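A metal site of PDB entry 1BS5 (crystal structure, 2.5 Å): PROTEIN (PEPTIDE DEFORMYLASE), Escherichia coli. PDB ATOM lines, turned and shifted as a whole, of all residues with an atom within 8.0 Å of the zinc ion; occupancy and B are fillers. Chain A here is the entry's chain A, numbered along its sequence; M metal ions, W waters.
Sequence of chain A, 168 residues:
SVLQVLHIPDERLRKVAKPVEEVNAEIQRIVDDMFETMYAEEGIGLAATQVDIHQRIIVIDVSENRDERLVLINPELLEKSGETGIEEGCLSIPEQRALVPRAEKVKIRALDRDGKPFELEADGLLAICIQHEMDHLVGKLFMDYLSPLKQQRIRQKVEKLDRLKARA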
ATOM      1  N   VAL A   5      30.767  -0.922  16.103  1.00  0.00           N
ATOM      2  CA  VAL A   5      29.468  -0.928  16.782  1.00  0.00           C
ATOM      3  C   VAL A   5      29.638  -0.272  18.145  1.00  0.00           C
ATOM      4  O   VAL A   5      30.557  -0.614  18.878  1.00  0.00           O
ATOM      5  CB  VAL A   5      28.966  -2.381  16.988  1.00  0.00           C
ATOM      6  CG1 VAL A   5      27.711  -2.404  17.840  1.00  0.00           C
ATOM      7  CG2 VAL A   5      28.708  -3.042  15.649  1.00  0.00           C
ATOM      8  N   GLY A  45      20.294  -8.926  13.871  1.00  0.00           N
ATOM      9  CA  GLY A  45      19.809  -7.625  13.463  1.00  0.00           C
ATOM     10  C   GLY A  45      20.810  -6.530  13.779  1.00  0.00           C
ATOM     11  O   GLY A  45      21.620  -6.676  14.688  1.00  0.00           O
ATOM     12  N   LEU A  46      20.769  -5.446  13.003  1.00  0.00           N
ATOM     13  CA  LEU A  46      21.555  -4.240  13.299  1.00  0.00           C
ATOM     14  C   LEU A  46      20.813  -2.994  12.776  1.00  0.00           C
ATOM     15  O   LEU A  46      20.183  -3.029  11.712  1.00  0.00           O
ATOM     16  CB  LEU A  46      22.943  -4.344  12.639  1.00  0.00           C
ATOM     17  CG  LEU A  46      24.097  -3.434  13.038  1.00  0.00           C
ATOM     18  CD1 LEU A  46      24.696  -3.806  14.388  1.00  0.00           C
ATOM     19  CD2 LEU A  46      25.141  -3.620  11.974  1.00  0.00           C
ATOM     20  N   ALA A  47      20.732  -1.976  13.626  1.00  0.00           N
ATOM     21  CA  ALA A  47      20.162  -0.681  13.270  1.00  0.00           C
ATOM     22  C   ALA A  47      21.298   0.301  12.973  1.00  0.00           C
ATOM     23  O   ALA A  47      22.346   0.273  13.658  1.00  0.00           O
ATOM     24  CB  ALA A  47      19.296  -0.152  14.415  1.00  0.00           C
ATOM     25  N   GLN A  50      23.368   2.185  15.652  1.00  0.00           N
ATOM     26  CA  GLN A  50      24.409   1.430  16.350  1.00  0.00           C
ATOM     27  C   GLN A  50      25.794   1.577  15.727  1.00  0.00           C
ATOM     28  O   GLN A  50      26.803   1.295  16.373  1.00  0.00           O
ATOM     29  CB  GLN A  50      24.049  -0.052  16.378  1.00  0.00           C
ATOM     30  CG  GLN A  50      22.933  -0.379  17.314  1.00  0.00           C
ATOM     31  CD  GLN A  50      22.544  -1.835  17.217  1.00  0.00           C
ATOM     32  OE1 GLN A  50      21.725  -2.201  16.379  1.00  0.00           O
ATOM     33  NE2 GLN A  50      23.213  -2.690  17.983  1.00  0.00           N
ATOM     34  N   GLU A  88      16.606 -11.665  24.958  1.00  0.00           N
ATOM     35  CA  GLU A  88      17.231 -10.887  23.870  1.00  0.00           C
ATOM     36  C   GLU A  88      18.674 -10.488  24.137  1.00  0.00           C
ATOM     37  O   GLU A  88      19.093 -10.307  25.273  1.00  0.00           O
ATOM     38  CB  GLU A  88      16.428  -9.611  23.617  1.00  0.00           C
ATOM     39  CG  GLU A  88      15.186  -9.820  22.831  1.00  0.00           C
ATOM     40  CD  GLU A  88      14.387  -8.554  22.684  1.00  0.00           C
ATOM     41  OE1 GLU A  88      14.979  -7.459  22.552  1.00  0.00           O
ATOM     42  OE2 GLU A  88      13.152  -8.651  22.694  1.00  0.00           O
ATOM     43  N   GLY A  89      19.420 -10.277  23.063  1.00  0.00           N
ATOM     44  CA  GLY A  89      20.715  -9.655  23.197  1.00  0.00           C
ATOM     45  C   GLY A  89      20.802  -8.494  22.237  1.00  0.00           C
ATOM     46  O   GLY A  89      19.839  -8.191  21.494  1.00  0.00           O
ATOM     47  N   CYS A  90      22.013  -7.928  22.138  1.00  0.00           N
ATOM     48  CA  CYS A  90      22.249  -6.701  21.369  1.00  0.00           C
ATOM     49  C   CYS A  90      23.760  -6.523  21.216  1.00  0.00           C
ATOM     50  O   CYS A  90      24.501  -6.556  22.204  1.00  0.00           O
ATOM     51  CB  CYS A  90      21.639  -5.495  22.105  1.00  0.00           C
ATOM     52  SG  CYS A  90      21.581  -3.975  21.133  1.00  0.00           S
ATOM     53  N   LEU A  91      24.206  -6.289  19.989  1.00  0.00           N
ATOM     54  CA  LEU A  91      25.622  -6.057  19.746  1.00  0.00           C
ATOM     55  C   LEU A  91      26.147  -4.842  20.504  1.00  0.00           C
ATOM     56  O   LEU A  91      27.330  -4.756  20.762  1.00  0.00           O
ATOM     57  CB  LEU A  91      25.890  -5.943  18.239  1.00  0.00           C
ATOM     58  CG  LEU A  91      25.737  -7.232  17.413  1.00  0.00           C
ATOM     59  CD1 LEU A  91      26.091  -7.027  15.940  1.00  0.00           C
ATOM     60  CD2 LEU A  91      26.638  -8.284  18.005  1.00  0.00           C
ATOM     61  N   SER A  92      25.247  -3.931  20.893  1.00  0.00           N
ATOM     62  CA  SER A  92      25.635  -2.717  21.622  1.00  0.00           C
ATOM     63  C   SER A  92      25.619  -2.891  23.145  1.00  0.00           C
ATOM     64  O   SER A  92      26.043  -2.003  23.899  1.00  0.00           O
ATOM     65  CB  SER A  92      24.723  -1.564  21.238  1.00  0.00           C
ATOM     66  OG  SER A  92      24.803  -1.299  19.844  1.00  0.00           O
ATOM     67  N   ILE A  93      25.055  -4.002  23.601  1.00  0.00           N
ATOM     68  CA  ILE A  93      25.101  -4.362  25.018  1.00  0.00           C
ATOM     69  C   ILE A  93      25.749  -5.735  25.152  1.00  0.00           C
ATOM     70  O   ILE A  93      25.057  -6.757  25.273  1.00  0.00           O
ATOM     71  CB  ILE A  93      23.682  -4.401  25.645  1.00  0.00           C
ATOM     72  CG1 ILE A  93      23.004  -3.049  25.471  1.00  0.00           C
ATOM     73  CG2 ILE A  93      23.749  -4.737  27.123  1.00  0.00           C
ATOM     74  CD1 ILE A  93      21.531  -3.076  25.720  1.00  0.00           C
ATOM     75  N   ARG A 102       7.350  -7.972  24.293  1.00  0.00           N
ATOM     76  CA  ARG A 102       7.176  -7.584  22.904  1.00  0.00           C
ATOM     77  C   ARG A 102       5.792  -7.964  22.446  1.00  0.00           C
ATOM     78  O   ARG A 102       5.138  -8.794  23.054  1.00  0.00           O
ATOM     79  CB  ARG A 102       8.183  -8.297  22.007  1.00  0.00           C
ATOM     80  CG  ARG A 102       9.629  -8.007  22.266  1.00  0.00           C
ATOM     81  CD  ARG A 102      10.005  -6.571  21.909  1.00  0.00           C
ATOM     82  NE  ARG A 102      11.412  -6.356  22.222  1.00  0.00           N
ATOM     83  CZ  ARG A 102      12.033  -5.186  22.230  1.00  0.00           C
ATOM     84  NH1 ARG A 102      11.366  -4.054  21.976  1.00  0.00           N
ATOM     85  NH2 ARG A 102      13.326  -5.156  22.527  1.00  0.00           N
ATOM     86  N   CYS A 129      12.515  -9.253  16.638  1.00  0.00           N
ATOM     87  CA  CYS A 129      13.621  -8.587  15.960  1.00  0.00           C
ATOM     88  C   CYS A 129      13.273  -7.202  15.460  1.00  0.00           C
ATOM     89  O   CYS A 129      13.995  -6.240  15.691  1.00  0.00           O
ATOM     90  CB  CYS A 129      14.045  -9.417  14.761  1.00  0.00           C
ATOM     91  SG  CYS A 129      15.489 -10.354  15.082  1.00  0.00           S
ATOM     92  N   HIS A 132      12.786  -4.740  18.325  1.00  0.00           N
ATOM     93  CA  HIS A 132      14.047  -4.400  18.989  1.00  0.00           C
ATOM     94  C   HIS A 132      14.798  -3.396  18.115  1.00  0.00           C
ATOM     95  O   HIS A 132      15.384  -2.436  18.609  1.00  0.00           O
ATOM     96  CB  HIS A 132      14.864  -5.678  19.176  1.00  0.00           C
ATOM     97  CG  HIS A 132      16.280  -5.466  19.659  1.00  0.00           C
ATOM     98  ND1 HIS A 132      16.776  -6.079  20.786  1.00  0.00           N
ATOM     99  CD2 HIS A 132      17.327  -4.802  19.101  1.00  0.00           C
ATOM    100  CE1 HIS A 132      18.056  -5.801  20.913  1.00  0.00           C
ATOM    101  NE2 HIS A 132      18.424  -5.039  19.895  1.00  0.00           N
ATOM    102  N   GLU A 133      14.832  -3.652  16.809  1.00  0.00           N
ATOM    103  CA  GLU A 133      15.635  -2.845  15.908  1.00  0.00           C
ATOM    104  C   GLU A 133      15.003  -1.474  15.722  1.00  0.00           C
ATOM    105  O   GLU A 133      15.670  -0.457  15.838  1.00  0.00           O
ATOM    106  CB  GLU A 133      15.784  -3.544  14.539  1.00  0.00           C
ATOM    107  CG  GLU A 133      16.750  -4.724  14.498  1.00  0.00           C
ATOM    108  CD  GLU A 133      18.009  -4.497  15.282  1.00  0.00           C
ATOM    109  OE1 GLU A 133      18.577  -3.396  15.238  1.00  0.00           O
ATOM    110  OE2 GLU A 133      18.470  -5.447  15.935  1.00  0.00           O
ATOM    111  N   ASP A 135      13.291   0.088  17.728  1.00  0.00           N
ATOM    112  CA  ASP A 135      13.509   0.800  18.986  1.00  0.00           C
ATOM    113  C   ASP A 135      14.810   1.574  18.920  1.00  0.00           C
ATOM    114  O   ASP A 135      14.949   2.612  19.555  1.00  0.00           O
ATOM    115  CB  ASP A 135      13.587  -0.177  20.149  1.00  0.00           C
ATOM    116  CG  ASP A 135      12.253  -0.387  20.838  1.00  0.00           C
ATOM    117  OD1 ASP A 135      11.220   0.125  20.358  1.00  0.00           O
ATOM    118  OD2 ASP A 135      12.246  -1.090  21.882  1.00  0.00           O
ATOM    119  N   HIS A 136      15.814   0.991  18.286  1.00  0.00           N
ATOM    120  CA  HIS A 136      17.125   1.616  18.184  1.00  0.00           C
ATOM    121  C   HIS A 136      17.006   2.942  17.488  1.00  0.00           C
ATOM    122  O   HIS A 136      17.531   3.932  17.961  1.00  0.00           O
ATOM    123  CB  HIS A 136      18.086   0.744  17.390  1.00  0.00           C
ATOM    124  CG  HIS A 136      18.844  -0.252  18.218  1.00  0.00           C
ATOM    125  ND1 HIS A 136      19.601   0.100  19.311  1.00  0.00           N
ATOM    126  CD2 HIS A 136      18.945  -1.597  18.112  1.00  0.00           C
ATOM    127  CE1 HIS A 136      20.123  -0.985  19.851  1.00  0.00           C
ATOM    128  NE2 HIS A 136      19.741  -2.032  19.143  1.00  0.00           N
ATOM    129  N   LYS A 140      16.005   3.912  21.913  1.00  0.00           N
ATOM    130  CA  LYS A 140      15.536   2.960  22.935  1.00  0.00           C
ATOM    131  C   LYS A 140      16.360   1.646  22.909  1.00  0.00           C
ATOM    132  O   LYS A 140      16.542   1.033  21.850  1.00  0.00           O
ATOM    133  CB  LYS A 140      14.078   2.631  22.670  1.00  0.00           C
ATOM    134  CG  LYS A 140      13.153   2.945  23.764  1.00  0.00           C
ATOM    135  CD  LYS A 140      12.843   1.687  24.555  1.00  0.00           C
ATOM    136  CE  LYS A 140      11.571   1.870  25.402  1.00  0.00           C
ATOM    137  NZ  LYS A 140      10.311   2.029  24.555  1.00  0.00           N
ATOM    138  N   LEU A 141      16.858   1.221  24.064  1.00  0.00           N
ATOM    139  CA  LEU A 141      17.580  -0.047  24.162  1.00  0.00           C
ATOM    140  C   LEU A 141      16.729  -0.987  25.004  1.00  0.00           C
ATOM    141  O   LEU A 141      15.891  -0.522  25.784  1.00  0.00           O
ATOM    142  CB  LEU A 141      18.950   0.135  24.835  1.00  0.00           C
ATOM    143  CG  LEU A 141      19.794   1.311  24.335  1.00  0.00           C
ATOM    144  CD1 LEU A 141      20.953   1.541  25.258  1.00  0.00           C
ATOM    145  CD2 LEU A 141      20.276   1.035  22.932  1.00  0.00           C
ATOM    146  N   PHE A 142      16.951  -2.289  24.871  1.00  0.00           N
ATOM    147  CA  PHE A 142      16.089  -3.269  25.529  1.00  0.00           C
ATOM    148  C   PHE A 142      16.170  -3.233  27.057  1.00  0.00           C
ATOM    149  O   PHE A 142      15.173  -3.519  27.731  1.00  0.00           O
ATOM    150  CB  PHE A 142      16.317  -4.698  24.990  1.00  0.00           C
ATOM    151  CG  PHE A 142      17.563  -5.372  25.468  1.00  0.00           C
ATOM    152  CD1 PHE A 142      17.681  -5.815  26.791  1.00  0.00           C
ATOM    153  CD2 PHE A 142      18.575  -5.700  24.577  1.00  0.00           C
ATOM    154  CE1 PHE A 142      18.778  -6.542  27.206  1.00  0.00           C
ATOM    155  CE2 PHE A 142      19.687  -6.446  24.998  1.00  0.00           C
ATOM    156  CZ  PHE A 142      19.776  -6.852  26.325  1.00  0.00           C
HETATM  157 ZN    ZN M   1      20.173  -4.105  19.533  1.00  0.00          ZN
HETATM  158  O   HOH W   1      20.459  -4.600  17.361  1.00  0.00           O
HETATM  159  O   HOH W   2      19.057  -3.051  22.271  1.00  0.00           O
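ND1 of His 132 is in hydrogen-bond range of OE1 of Glu 88, at 2.9 Å. SG of Cys 90 lies close to NE2 of Gln 50 (3.8 Å). The side-chain sulfur of Cys 90 sits close to the backbone NH of Ser 92. The side-chain amide oxygen (OE1) of Gln 50 sits close to a ring nitrogen (NE2) of His 136, 3.4 Å away. The side-chain amide nitrogen of Gln 50 sits at hydrogen-bond distance from the side-chain hydroxyl of Ser 92 (2.8 Å). The backbone NH of Ala 47 is in hydrogen-bond range of the side-chain amide oxygen of Gln 50 (2.9 Å).
Merely in contact with the zinc ion: Gln 50 (3.7 Å). Four residues have an atom within 4 Å of the zinc ion: Gln 50, Cys 90, His 132 and His 136.
The zinc ion is bound by a ring nitrogen (NE2) of His 132 (2.0 Å), the side-chain sulfur of Cys 90 (2.1 Å), a ring nitrogen (NE2) of His 136 (2.2 Å) and water W1 (2.2 Å). The zinc ion has four donor atoms within binding distance.
Water W1 bridges OE2 of Glu 133 (2.6 Å) and OE1 of Gln 50 (2.9 Å).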
